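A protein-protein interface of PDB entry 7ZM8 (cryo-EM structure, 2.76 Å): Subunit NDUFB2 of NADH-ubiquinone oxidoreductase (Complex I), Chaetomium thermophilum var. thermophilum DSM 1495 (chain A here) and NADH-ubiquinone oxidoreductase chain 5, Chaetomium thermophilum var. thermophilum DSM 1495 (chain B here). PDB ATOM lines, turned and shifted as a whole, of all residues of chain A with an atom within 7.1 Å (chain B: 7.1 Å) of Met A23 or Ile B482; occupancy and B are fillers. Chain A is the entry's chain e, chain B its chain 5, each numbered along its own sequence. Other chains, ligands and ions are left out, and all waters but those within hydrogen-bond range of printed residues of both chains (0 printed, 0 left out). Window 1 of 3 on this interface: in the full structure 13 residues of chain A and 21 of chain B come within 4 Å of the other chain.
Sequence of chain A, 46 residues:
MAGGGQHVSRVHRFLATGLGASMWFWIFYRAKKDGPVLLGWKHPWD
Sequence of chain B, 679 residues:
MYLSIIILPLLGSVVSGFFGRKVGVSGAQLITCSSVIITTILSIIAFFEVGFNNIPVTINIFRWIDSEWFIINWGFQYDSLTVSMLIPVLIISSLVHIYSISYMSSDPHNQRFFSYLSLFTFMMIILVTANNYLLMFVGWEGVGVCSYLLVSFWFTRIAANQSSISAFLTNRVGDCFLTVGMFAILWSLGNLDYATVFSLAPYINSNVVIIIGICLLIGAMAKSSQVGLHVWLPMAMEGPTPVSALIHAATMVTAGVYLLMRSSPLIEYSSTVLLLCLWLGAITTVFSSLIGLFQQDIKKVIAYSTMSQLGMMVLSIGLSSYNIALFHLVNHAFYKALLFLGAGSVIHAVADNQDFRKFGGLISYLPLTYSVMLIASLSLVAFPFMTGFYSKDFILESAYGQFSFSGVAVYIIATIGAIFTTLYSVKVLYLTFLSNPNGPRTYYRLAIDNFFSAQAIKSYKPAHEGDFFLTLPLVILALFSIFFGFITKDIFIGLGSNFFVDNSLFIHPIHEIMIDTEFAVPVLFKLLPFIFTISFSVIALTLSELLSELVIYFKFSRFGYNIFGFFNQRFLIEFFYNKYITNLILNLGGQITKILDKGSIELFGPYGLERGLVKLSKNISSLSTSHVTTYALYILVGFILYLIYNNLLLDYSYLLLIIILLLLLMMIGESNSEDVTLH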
ATOM      1  N   THR A  17      -5.191  -0.512  15.735  1.00  0.00           N
ATOM      2  CA  THR A  17      -6.295  -1.159  15.038  1.00  0.00           C
ATOM      3  C   THR A  17      -7.343  -1.686  16.007  1.00  0.00           C
ATOM      4  O   THR A  17      -8.519  -1.787  15.647  1.00  0.00           O
ATOM      5  CB  THR A  17      -5.777  -2.283  14.143  1.00  0.00           C
ATOM      6  OG1 THR A  17      -6.853  -2.790  13.345  1.00  0.00           O
ATOM      7  CG2 THR A  17      -5.185  -3.413  14.968  1.00  0.00           C
ATOM      8  N   GLY A  18      -6.939  -2.040  17.227  1.00  0.00           N
ATOM      9  CA  GLY A  18      -7.914  -2.458  18.217  1.00  0.00           C
ATOM     10  C   GLY A  18      -8.826  -1.325  18.636  1.00  0.00           C
ATOM     11  O   GLY A  18     -10.038  -1.507  18.771  1.00  0.00           O
ATOM     12  N   LEU A  19      -8.256  -0.140  18.850  1.00  0.00           N
ATOM     13  CA  LEU A  19      -9.070   1.025  19.168  1.00  0.00           C
ATOM     14  C   LEU A  19      -9.962   1.398  17.998  1.00  0.00           C
ATOM     15  O   LEU A  19     -11.102   1.836  18.194  1.00  0.00           O
ATOM     16  CB  LEU A  19      -8.176   2.196  19.559  1.00  0.00           C
ATOM     17  CG  LEU A  19      -7.588   2.036  20.956  1.00  0.00           C
ATOM     18  CD1 LEU A  19      -6.458   3.016  21.195  1.00  0.00           C
ATOM     19  CD2 LEU A  19      -8.677   2.183  21.994  1.00  0.00           C
ATOM     20  N   GLY A  20      -9.454   1.252  16.776  1.00  0.00           N
ATOM     21  CA  GLY A  20     -10.289   1.465  15.610  1.00  0.00           C
ATOM     22  C   GLY A  20     -11.389   0.430  15.488  1.00  0.00           C
ATOM     23  O   GLY A  20     -12.538   0.766  15.196  1.00  0.00           O
ATOM     24  N   ALA A  21     -11.054  -0.841  15.703  1.00  0.00           N
ATOM     25  CA  ALA A  21     -12.068  -1.885  15.696  1.00  0.00           C
ATOM     26  C   ALA A  21     -13.000  -1.792  16.897  1.00  0.00           C
ATOM     27  O   ALA A  21     -14.059  -2.424  16.892  1.00  0.00           O
ATOM     28  CB  ALA A  21     -11.410  -3.263  15.653  1.00  0.00           C
ATOM     29  N   SER A  22     -12.629  -1.029  17.927  1.00  0.00           N
ATOM     30  CA  SER A  22     -13.585  -0.714  18.980  1.00  0.00           C
ATOM     31  C   SER A  22     -14.764   0.060  18.411  1.00  0.00           C
ATOM     32  O   SER A  22     -15.922  -0.325  18.594  1.00  0.00           O
ATOM     33  CB  SER A  22     -12.899   0.071  20.096  1.00  0.00           C
ATOM     34  OG  SER A  22     -12.046  -0.765  20.856  1.00  0.00           O
ATOM     35  N   MET A  23     -14.447   1.141  17.685  1.00  0.00           N
ATOM     36  CA  MET A  23     -15.500   1.874  16.939  1.00  0.00           C
ATOM     37  C   MET A  23     -15.798   0.996  15.727  1.00  0.00           C
ATOM     38  O   MET A  23     -15.113  -0.027  15.568  1.00  0.00           O
ATOM     39  CB  MET A  23     -14.957   3.185  16.373  1.00  0.00           C
ATOM     40  CG  MET A  23     -14.851   4.325  17.342  1.00  0.00           C
ATOM     41  SD  MET A  23     -14.455   5.811  16.388  1.00  0.00           S
ATOM     42  CE  MET A  23     -13.443   5.104  15.091  1.00  0.00           C
ATOM     43  N   TRP A  24     -16.814   1.324  14.938  1.00  0.00           N
ATOM     44  CA  TRP A  24     -17.082   0.559  13.692  1.00  0.00           C
ATOM     45  C   TRP A  24     -17.588  -0.823  14.091  1.00  0.00           C
ATOM     46  O   TRP A  24     -17.671  -1.696  13.228  1.00  0.00           O
ATOM     47  CB  TRP A  24     -15.875   0.507  12.740  1.00  0.00           C
ATOM     48  CG  TRP A  24     -15.277   1.835  12.392  1.00  0.00           C
ATOM     49  CD1 TRP A  24     -13.956   2.172  12.452  1.00  0.00           C
ATOM     50  CD2 TRP A  24     -15.969   3.007  11.926  1.00  0.00           C
ATOM     51  NE1 TRP A  24     -13.777   3.468  12.055  1.00  0.00           N
ATOM     52  CE2 TRP A  24     -14.993   4.007  11.727  1.00  0.00           C
ATOM     53  CE3 TRP A  24     -17.306   3.312  11.653  1.00  0.00           C
ATOM     54  CZ2 TRP A  24     -15.319   5.285  11.277  1.00  0.00           C
ATOM     55  CZ3 TRP A  24     -17.627   4.575  11.208  1.00  0.00           C
ATOM     56  CH2 TRP A  24     -16.645   5.546  11.022  1.00  0.00           C
ATOM     57  N   PHE A  25     -17.783  -1.056  15.380  1.00  0.00           N
ATOM     58  CA  PHE A  25     -18.445  -2.302  15.827  1.00  0.00           C
ATOM     59  C   PHE A  25     -19.538  -1.744  16.715  1.00  0.00           C
ATOM     60  O   PHE A  25     -20.701  -2.128  16.553  1.00  0.00           O
ATOM     61  CB  PHE A  25     -17.496  -3.246  16.562  1.00  0.00           C
ATOM     62  CG  PHE A  25     -18.097  -4.608  16.794  1.00  0.00           C
ATOM     63  CD1 PHE A  25     -18.083  -5.568  15.795  1.00  0.00           C
ATOM     64  CD2 PHE A  25     -18.709  -4.922  17.998  1.00  0.00           C
ATOM     65  CE1 PHE A  25     -18.647  -6.816  16.001  1.00  0.00           C
ATOM     66  CE2 PHE A  25     -19.274  -6.170  18.201  1.00  0.00           C
ATOM     67  CZ  PHE A  25     -19.242  -7.115  17.204  1.00  0.00           C
ATOM     68  N   TRP A  26     -19.148  -0.828  17.603  1.00  0.00           N
ATOM     69  CA  TRP A  26     -20.147  -0.110  18.427  1.00  0.00           C
ATOM     70  C   TRP A  26     -20.990   0.718  17.465  1.00  0.00           C
ATOM     71  O   TRP A  26     -22.207   0.740  17.632  1.00  0.00           O
ATOM     72  CB  TRP A  26     -19.405   0.790  19.417  1.00  0.00           C
ATOM     73  CG  TRP A  26     -20.274   1.549  20.370  1.00  0.00           C
ATOM     74  CD1 TRP A  26     -20.409   2.904  20.458  1.00  0.00           C
ATOM     75  CD2 TRP A  26     -21.113   0.994  21.399  1.00  0.00           C
ATOM     76  NE1 TRP A  26     -21.275   3.230  21.465  1.00  0.00           N
ATOM     77  CE2 TRP A  26     -21.721   2.080  22.061  1.00  0.00           C
ATOM     78  CE3 TRP A  26     -21.408  -0.305  21.825  1.00  0.00           C
ATOM     79  CZ2 TRP A  26     -22.610   1.900  23.117  1.00  0.00           C
ATOM     80  CZ3 TRP A  26     -22.287  -0.481  22.868  1.00  0.00           C
ATOM     81  CH2 TRP A  26     -22.880   0.609  23.504  1.00  0.00           C
ATOM     82  N   ILE A  27     -20.347   1.335  16.473  1.00  0.00           N
ATOM     83  CA  ILE A  27     -21.072   2.228  15.523  1.00  0.00           C
ATOM     84  C   ILE A  27     -22.196   1.441  14.838  1.00  0.00           C
ATOM     85  O   ILE A  27     -23.346   1.900  14.922  1.00  0.00           O
ATOM     86  CB  ILE A  27     -20.103   2.885  14.521  1.00  0.00           C
ATOM     87  CG1 ILE A  27     -19.075   3.766  15.235  1.00  0.00           C
ATOM     88  CG2 ILE A  27     -20.865   3.667  13.462  1.00  0.00           C
ATOM     89  CD1 ILE A  27     -19.687   4.813  16.133  1.00  0.00           C
ATOM     90  N   PHE A  28     -21.886   0.317  14.184  1.00  0.00           N
ATOM     91  CA  PHE A  28     -22.956  -0.396  13.501  1.00  0.00           C
ATOM     92  C   PHE A  28     -23.839  -1.190  14.450  1.00  0.00           C
ATOM     93  O   PHE A  28     -25.002  -1.443  14.124  1.00  0.00           O
ATOM     94  CB  PHE A  28     -22.409  -1.297  12.392  1.00  0.00           C
ATOM     95  CG  PHE A  28     -21.229  -0.732  11.667  1.00  0.00           C
ATOM     96  CD1 PHE A  28     -21.321   0.491  11.030  1.00  0.00           C
ATOM     97  CD2 PHE A  28     -20.069  -1.452  11.535  1.00  0.00           C
ATOM     98  CE1 PHE A  28     -20.248   1.010  10.336  1.00  0.00           C
ATOM     99  CE2 PHE A  28     -18.995  -0.939  10.832  1.00  0.00           C
ATOM    100  CZ  PHE A  28     -19.081   0.289  10.240  1.00  0.00           C
ATOM    101  N   LEU B 338      -8.105  14.358  24.722  1.00  0.00           N
ATOM    102  CA  LEU B 338      -7.520  13.346  23.810  1.00  0.00           C
ATOM    103  C   LEU B 338      -6.811  14.038  22.647  1.00  0.00           C
ATOM    104  O   LEU B 338      -5.642  13.699  22.410  1.00  0.00           O
ATOM    105  CB  LEU B 338      -8.647  12.449  23.301  1.00  0.00           C
ATOM    106  CG  LEU B 338      -8.193  11.139  22.670  1.00  0.00           C
ATOM    107  CD1 LEU B 338      -7.251  10.408  23.608  1.00  0.00           C
ATOM    108  CD2 LEU B 338      -9.383  10.266  22.316  1.00  0.00           C
ATOM    109  N   SER B 371      -5.128   6.996  14.894  1.00  0.00           N
ATOM    110  CA  SER B 371      -6.413   6.376  15.188  1.00  0.00           C
ATOM    111  C   SER B 371      -7.069   7.022  16.394  1.00  0.00           C
ATOM    112  O   SER B 371      -8.272   7.293  16.384  1.00  0.00           O
ATOM    113  CB  SER B 371      -6.228   4.881  15.421  1.00  0.00           C
ATOM    114  OG  SER B 371      -5.761   4.636  16.731  1.00  0.00           O
ATOM    115  N   LEU B 374      -8.368  10.197  15.431  1.00  0.00           N
ATOM    116  CA  LEU B 374      -9.574   9.910  14.665  1.00  0.00           C
ATOM    117  C   LEU B 374     -10.742   9.585  15.589  1.00  0.00           C
ATOM    118  O   LEU B 374     -11.880   9.969  15.312  1.00  0.00           O
ATOM    119  CB  LEU B 374      -9.304   8.763  13.691  1.00  0.00           C
ATOM    120  CG  LEU B 374     -10.368   8.400  12.655  1.00  0.00           C
ATOM    121  CD1 LEU B 374     -10.786   9.611  11.852  1.00  0.00           C
ATOM    122  CD2 LEU B 374      -9.839   7.307  11.752  1.00  0.00           C
ATOM    123  N   ILE B 375     -10.475   8.876  16.693  1.00  0.00           N
ATOM    124  CA  ILE B 375     -11.493   8.674  17.724  1.00  0.00           C
ATOM    125  C   ILE B 375     -12.014  10.020  18.202  1.00  0.00           C
ATOM    126  O   ILE B 375     -13.226  10.253  18.276  1.00  0.00           O
ATOM    127  CB  ILE B 375     -10.917   7.868  18.905  1.00  0.00           C
ATOM    128  CG1 ILE B 375     -10.371   6.499  18.491  1.00  0.00           C
ATOM    129  CG2 ILE B 375     -11.960   7.704  20.003  1.00  0.00           C
ATOM    130  CD1 ILE B 375     -11.374   5.552  17.996  1.00  0.00           C
ATOM    131  N   ALA B 376     -11.095  10.930  18.526  1.00  0.00           N
ATOM    132  CA  ALA B 376     -11.466  12.211  19.106  1.00  0.00           C
ATOM    133  C   ALA B 376     -12.178  13.098  18.098  1.00  0.00           C
ATOM    134  O   ALA B 376     -13.109  13.828  18.456  1.00  0.00           O
ATOM    135  CB  ALA B 376     -10.222  12.906  19.647  1.00  0.00           C
ATOM    136  N   LEU B 378     -14.047  12.231  15.551  1.00  0.00           N
ATOM    137  CA  LEU B 378     -15.393  11.776  15.234  1.00  0.00           C
ATOM    138  C   LEU B 378     -16.393  12.166  16.311  1.00  0.00           C
ATOM    139  O   LEU B 378     -17.566  12.394  16.007  1.00  0.00           O
ATOM    140  CB  LEU B 378     -15.414  10.268  15.016  1.00  0.00           C
ATOM    141  CG  LEU B 378     -14.851   9.785  13.688  1.00  0.00           C
ATOM    142  CD1 LEU B 378     -14.871   8.286  13.656  1.00  0.00           C
ATOM    143  CD2 LEU B 378     -15.669  10.352  12.554  1.00  0.00           C
ATOM    144  N   SER B 379     -15.962  12.239  17.566  1.00  0.00           N
ATOM    145  CA  SER B 379     -16.852  12.723  18.612  1.00  0.00           C
ATOM    146  C   SER B 379     -16.880  14.245  18.665  1.00  0.00           C
ATOM    147  O   SER B 379     -17.863  14.826  19.132  1.00  0.00           O
ATOM    148  CB  SER B 379     -16.438  12.143  19.964  1.00  0.00           C
ATOM    149  OG  SER B 379     -15.043  12.254  20.156  1.00  0.00           O
ATOM    150  N   PHE B 383     -20.174  12.537  15.307  1.00  0.00           N
ATOM    151  CA  PHE B 383     -20.547  11.428  14.450  1.00  0.00           C
ATOM    152  C   PHE B 383     -21.484  10.501  15.218  1.00  0.00           C
ATOM    153  O   PHE B 383     -21.299  10.301  16.423  1.00  0.00           O
ATOM    154  CB  PHE B 383     -19.305  10.670  13.986  1.00  0.00           C
ATOM    155  CG  PHE B 383     -19.523   9.830  12.766  1.00  0.00           C
ATOM    156  CD1 PHE B 383     -19.344  10.358  11.508  1.00  0.00           C
ATOM    157  CD2 PHE B 383     -19.895   8.509  12.883  1.00  0.00           C
ATOM    158  CE1 PHE B 383     -19.537   9.588  10.393  1.00  0.00           C
ATOM    159  CE2 PHE B 383     -20.089   7.738  11.774  1.00  0.00           C
ATOM    160  CZ  PHE B 383     -19.911   8.275  10.526  1.00  0.00           C
ATOM    161  N   PHE B 385     -23.518   8.035  17.402  1.00  0.00           N
ATOM    162  CA  PHE B 385     -23.234   7.009  18.399  1.00  0.00           C
ATOM    163  C   PHE B 385     -21.864   7.164  19.045  1.00  0.00           C
ATOM    164  O   PHE B 385     -21.373   6.235  19.685  1.00  0.00           O
ATOM    165  CB  PHE B 385     -23.394   5.607  17.805  1.00  0.00           C
ATOM    166  CG  PHE B 385     -24.662   5.430  17.025  1.00  0.00           C
ATOM    167  CD1 PHE B 385     -25.890   5.580  17.634  1.00  0.00           C
ATOM    168  CD2 PHE B 385     -24.625   5.117  15.683  1.00  0.00           C
ATOM    169  CE1 PHE B 385     -27.057   5.417  16.919  1.00  0.00           C
ATOM    170  CE2 PHE B 385     -25.786   4.958  14.964  1.00  0.00           C
ATOM    171  CZ  PHE B 385     -27.004   5.105  15.583  1.00  0.00           C
ATOM    172  N   MET B 386     -21.236   8.320  18.903  1.00  0.00           N
ATOM    173  CA  MET B 386     -20.059   8.651  19.687  1.00  0.00           C
ATOM    174  C   MET B 386     -20.475   9.402  20.945  1.00  0.00           C
ATOM    175  O   MET B 386     -21.639   9.754  21.134  1.00  0.00           O
ATOM    176  CB  MET B 386     -19.069   9.484  18.873  1.00  0.00           C
ATOM    177  CG  MET B 386     -18.320   8.715  17.803  1.00  0.00           C
ATOM    178  SD  MET B 386     -17.723   7.139  18.427  1.00  0.00           S
ATOM    179  CE  MET B 386     -16.048   7.576  18.869  1.00  0.00           C
ATOM    180  N   THR B 387     -19.499   9.642  21.821  1.00  0.00           N
ATOM    181  CA  THR B 387     -19.799  10.333  23.068  1.00  0.00           C
ATOM    182  C   THR B 387     -20.317  11.740  22.804  1.00  0.00           C
ATOM    183  O   THR B 387     -21.285  12.180  23.433  1.00  0.00           O
ATOM    184  CB  THR B 387     -18.560  10.358  23.962  1.00  0.00           C
ATOM    185  OG1 THR B 387     -18.272   9.027  24.402  1.00  0.00           O
ATOM    186  CG2 THR B 387     -18.787  11.220  25.178  1.00  0.00           C
ATOM    187  N   GLY B 388     -19.712  12.448  21.850  1.00  0.00           N
ATOM    188  CA  GLY B 388     -20.151  13.795  21.533  1.00  0.00           C
ATOM    189  C   GLY B 388     -21.445  13.855  20.755  1.00  0.00           C
ATOM    190  O   GLY B 388     -22.045  14.929  20.652  1.00  0.00           O
ATOM    191  N   TYR B 390     -24.337  12.438  21.577  1.00  0.00           N
ATOM    192  CA  TYR B 390     -25.478  12.610  22.461  1.00  0.00           C
ATOM    193  C   TYR B 390     -25.494  13.965  23.142  1.00  0.00           C
ATOM    194  O   TYR B 390     -26.546  14.387  23.630  1.00  0.00           O
ATOM    195  CB  TYR B 390     -25.503  11.500  23.511  1.00  0.00           C
ATOM    196  CG  TYR B 390     -25.632  10.133  22.900  1.00  0.00           C
ATOM    197  CD1 TYR B 390     -24.512   9.409  22.535  1.00  0.00           C
ATOM    198  CD2 TYR B 390     -26.876   9.567  22.694  1.00  0.00           C
ATOM    199  CE1 TYR B 390     -24.626   8.162  21.970  1.00  0.00           C
ATOM    200  CE2 TYR B 390     -27.001   8.324  22.125  1.00  0.00           C
ATOM    201  CZ  TYR B 390     -25.874   7.620  21.770  1.00  0.00           C
ATOM    202  OH  TYR B 390     -25.998   6.371  21.208  1.00  0.00           O
ATOM    203  N   ILE B 476      -6.879   5.182  27.318  1.00  0.00           N
ATOM    204  CA  ILE B 476      -8.000   5.306  28.247  1.00  0.00           C
ATOM    205  C   ILE B 476      -8.994   6.348  27.748  1.00  0.00           C
ATOM    206  O   ILE B 476     -10.203   6.099  27.682  1.00  0.00           O
ATOM    207  CB  ILE B 476      -7.491   5.650  29.657  1.00  0.00           C
ATOM    208  CG1 ILE B 476      -6.555   4.558  30.168  1.00  0.00           C
ATOM    209  CG2 ILE B 476      -8.655   5.852  30.607  1.00  0.00           C
ATOM    210  CD1 ILE B 476      -5.804   4.947  31.407  1.00  0.00           C
ATOM    211  N   LEU B 477      -8.498   7.529  27.385  1.00  0.00           N
ATOM    212  CA  LEU B 477      -9.375   8.588  26.907  1.00  0.00           C
ATOM    213  C   LEU B 477     -10.073   8.215  25.610  1.00  0.00           C
ATOM    214  O   LEU B 477     -11.141   8.760  25.314  1.00  0.00           O
ATOM    215  CB  LEU B 477      -8.579   9.874  26.723  1.00  0.00           C
ATOM    216  CG  LEU B 477      -8.094  10.574  27.986  1.00  0.00           C
ATOM    217  CD1 LEU B 477      -7.426  11.890  27.633  1.00  0.00           C
ATOM    218  CD2 LEU B 477      -9.259  10.795  28.926  1.00  0.00           C
ATOM    219  N   ALA B 478      -9.488   7.314  24.823  1.00  0.00           N
ATOM    220  CA  ALA B 478     -10.165   6.811  23.636  1.00  0.00           C
ATOM    221  C   ALA B 478     -11.404   6.007  24.006  1.00  0.00           C
ATOM    222  O   ALA B 478     -12.458   6.161  23.384  1.00  0.00           O
ATOM    223  CB  ALA B 478      -9.199   5.966  22.809  1.00  0.00           C
ATOM    224  N   LEU B 479     -11.298   5.151  25.022  1.00  0.00           N
ATOM    225  CA  LEU B 479     -12.442   4.354  25.449  1.00  0.00           C
ATOM    226  C   LEU B 479     -13.560   5.232  25.985  1.00  0.00           C
ATOM    227  O   LEU B 479     -14.741   4.949  25.764  1.00  0.00           O
ATOM    228  CB  LEU B 479     -12.019   3.332  26.503  1.00  0.00           C
ATOM    229  CG  LEU B 479     -11.408   2.011  26.038  1.00  0.00           C
ATOM    230  CD1 LEU B 479     -12.429   1.221  25.238  1.00  0.00           C
ATOM    231  CD2 LEU B 479     -10.153   2.203  25.239  1.00  0.00           C
ATOM    232  N   PHE B 480     -13.209   6.292  26.715  1.00  0.00           N
ATOM    233  CA  PHE B 480     -14.210   7.268  27.130  1.00  0.00           C
ATOM    234  C   PHE B 480     -14.871   7.922  25.927  1.00  0.00           C
ATOM    235  O   PHE B 480     -16.098   8.056  25.878  1.00  0.00           O
ATOM    236  CB  PHE B 480     -13.571   8.335  28.012  1.00  0.00           C
ATOM    237  CG  PHE B 480     -13.523   7.978  29.462  1.00  0.00           C
ATOM    238  CD1 PHE B 480     -14.651   8.070  30.247  1.00  0.00           C
ATOM    239  CD2 PHE B 480     -12.338   7.577  30.045  1.00  0.00           C
ATOM    240  CE1 PHE B 480     -14.604   7.753  31.581  1.00  0.00           C
ATOM    241  CE2 PHE B 480     -12.285   7.260  31.382  1.00  0.00           C
ATOM    242  CZ  PHE B 480     -13.421   7.348  32.151  1.00  0.00           C
ATOM    243  N   SER B 481     -14.074   8.322  24.936  1.00  0.00           N
ATOM    244  CA  SER B 481     -14.580   9.043  23.778  1.00  0.00           C
ATOM    245  C   SER B 481     -15.512   8.206  22.920  1.00  0.00           C
ATOM    246  O   SER B 481     -16.189   8.766  22.054  1.00  0.00           O
ATOM    247  CB  SER B 481     -13.415   9.545  22.922  1.00  0.00           C
ATOM    248  OG  SER B 481     -12.680  10.552  23.587  1.00  0.00           O
ATOM    249  N   ILE B 482     -15.552   6.895  23.119  1.00  0.00           N
ATOM    250  CA  ILE B 482     -16.425   6.024  22.349  1.00  0.00           C
ATOM    251  C   ILE B 482     -17.698   5.683  23.110  1.00  0.00           C
ATOM    252  O   ILE B 482     -18.774   5.609  22.518  1.00  0.00           O
ATOM    253  CB  ILE B 482     -15.676   4.741  21.929  1.00  0.00           C
ATOM    254  CG1 ILE B 482     -14.416   5.081  21.139  1.00  0.00           C
ATOM    255  CG2 ILE B 482     -16.577   3.850  21.094  1.00  0.00           C
ATOM    256  CD1 ILE B 482     -13.626   3.873  20.732  1.00  0.00           C
ATOM    257  N   PHE B 483     -17.603   5.493  24.426  1.00  0.00           N
ATOM    258  CA  PHE B 483     -18.673   4.859  25.176  1.00  0.00           C
ATOM    259  C   PHE B 483     -19.269   5.698  26.294  1.00  0.00           C
ATOM    260  O   PHE B 483     -20.384   5.395  26.726  1.00  0.00           O
ATOM    261  CB  PHE B 483     -18.175   3.541  25.780  1.00  0.00           C
ATOM    262  CG  PHE B 483     -17.636   2.586  24.767  1.00  0.00           C
ATOM    263  CD1 PHE B 483     -18.473   2.001  23.839  1.00  0.00           C
ATOM    264  CD2 PHE B 483     -16.294   2.282  24.732  1.00  0.00           C
ATOM    265  CE1 PHE B 483     -17.981   1.127  22.904  1.00  0.00           C
ATOM    266  CE2 PHE B 483     -15.797   1.409  23.798  1.00  0.00           C
ATOM    267  CZ  PHE B 483     -16.642   0.830  22.885  1.00  0.00           C
ATOM    268  N   PHE B 484     -18.578   6.730  26.773  1.00  0.00           N
ATOM    269  CA  PHE B 484     -19.037   7.412  27.977  1.00  0.00           C
ATOM    270  C   PHE B 484     -20.374   8.106  27.758  1.00  0.00           C
ATOM    271  O   PHE B 484     -21.173   8.211  28.693  1.00  0.00           O
ATOM    272  CB  PHE B 484     -17.989   8.414  28.450  1.00  0.00           C
ATOM    273  CG  PHE B 484     -18.413   9.210  29.638  1.00  0.00           C
ATOM    274  CD1 PHE B 484     -18.323   8.673  30.907  1.00  0.00           C
ATOM    275  CD2 PHE B 484     -18.892  10.495  29.495  1.00  0.00           C
ATOM    276  CE1 PHE B 484     -18.710   9.398  32.007  1.00  0.00           C
ATOM    277  CE2 PHE B 484     -19.290  11.224  30.593  1.00  0.00           C
ATOM    278  CZ  PHE B 484     -19.197  10.675  31.852  1.00  0.00           C
ATOM    279  N   GLY B 485     -20.630   8.591  26.544  1.00  0.00           N
ATOM    280  CA  GLY B 485     -21.904   9.241  26.276  1.00  0.00           C
ATOM    281  C   GLY B 485     -23.078   8.293  26.399  1.00  0.00           C
ATOM    282  O   GLY B 485     -24.094   8.617  27.015  1.00  0.00           O
ATOM    283  N   PHE B 486     -22.953   7.104  25.811  1.00  0.00           N
ATOM    284  CA  PHE B 486     -24.031   6.124  25.887  1.00  0.00           C
ATOM    285  C   PHE B 486     -24.287   5.689  27.321  1.00  0.00           C
ATOM    286  O   PHE B 486     -25.439   5.576  27.748  1.00  0.00           O
ATOM    287  CB  PHE B 486     -23.697   4.910  25.021  1.00  0.00           C
ATOM    288  CG  PHE B 486     -24.801   3.903  24.942  1.00  0.00           C
ATOM    289  CD1 PHE B 486     -24.918   2.905  25.889  1.00  0.00           C
ATOM    290  CD2 PHE B 486     -25.718   3.951  23.916  1.00  0.00           C
ATOM    291  CE1 PHE B 486     -25.934   1.983  25.816  1.00  0.00           C
ATOM    292  CE2 PHE B 486     -26.737   3.033  23.840  1.00  0.00           C
ATOM    293  CZ  PHE B 486     -26.843   2.047  24.792  1.00  0.00           C
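The indole nitrogen of Trp A26 is in hydrogen-bond range of the backbone carbonyl oxygen of Phe B385 (3.5 Å).
The side-chain hydroxyl (OG) of Ser B379 sits at hydrogen-bond distance from the backbone carbonyl oxygen (O) of Ile B375 (3.3 Å). N of Phe B383 sits at hydrogen-bond distance from O of Leu B378 (2.7 Å). The side-chain hydroxyl (OG) of Ser A22 is in hydrogen-bond range of the backbone carbonyl oxygen (O) of Gly A18, 3.0 Å away.
Leu A19 touches Ile B375. CD2 of Leu A19 touches CD2 of Leu B479, at 3.6 Å. Met A23 touches Leu B378 (SD to CD1, 3.7 Å). Met B386 touches Met A23. Ile B482 touches Met A23. Trp A24 touches Leu B378 (CZ2 to CD1, 3.9 Å). NE1 of Trp A26 touches O of Ile B482 (3.6 Å). Phe B483 touches Trp A26 (CE1 to CG, 3.4 Å). Trp A26 touches Phe B486. Phe B385 touches Ile A27.
Of the printed residues of chain B, Leu A19 touches Ile B375, Ala B478 and Leu B479. Met A23 touches just these residues of chain B: Ile B375, Leu B378, Met B386 and Ile B482. Printed residues of chain B within 4 Å of Ile A27: Phe B385 and Met B386. Phe A28 touches none of the printed residues of chain B. Of chain A, only Ser A22, Met A23 and Trp A26 come within 4 Å of Ile B482. The nearest residue of chain B that does not touch Met A23 is Leu B374 (5.0 Å). The nearest residue of chain A that does not touch Ile B482 is Leu A19 (4.1 Å). The nearest printed residue of chain A that does not touch Met B386 is Trp A26 (5.4 Å).
Of the 24 printed residues of chain B, 9 touch a printed residue of chain A. Printed residues of chain B that touch a printed residue of chain A: Ile B375, Leu B378, Phe B385, Met B386, Ala B478, Leu B479, Ile B482, Phe B483 and Phe B486. Hydrophobic or aromatic side chains of chain A that line the printed part of chain B: Leu A19, Met A23, Trp A24, Trp A26 and Ile A27. Among the printed residues, no Asp or Glu carboxylate lies within 4 Å of a Lys or Arg side-chain nitrogen of the other chain.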
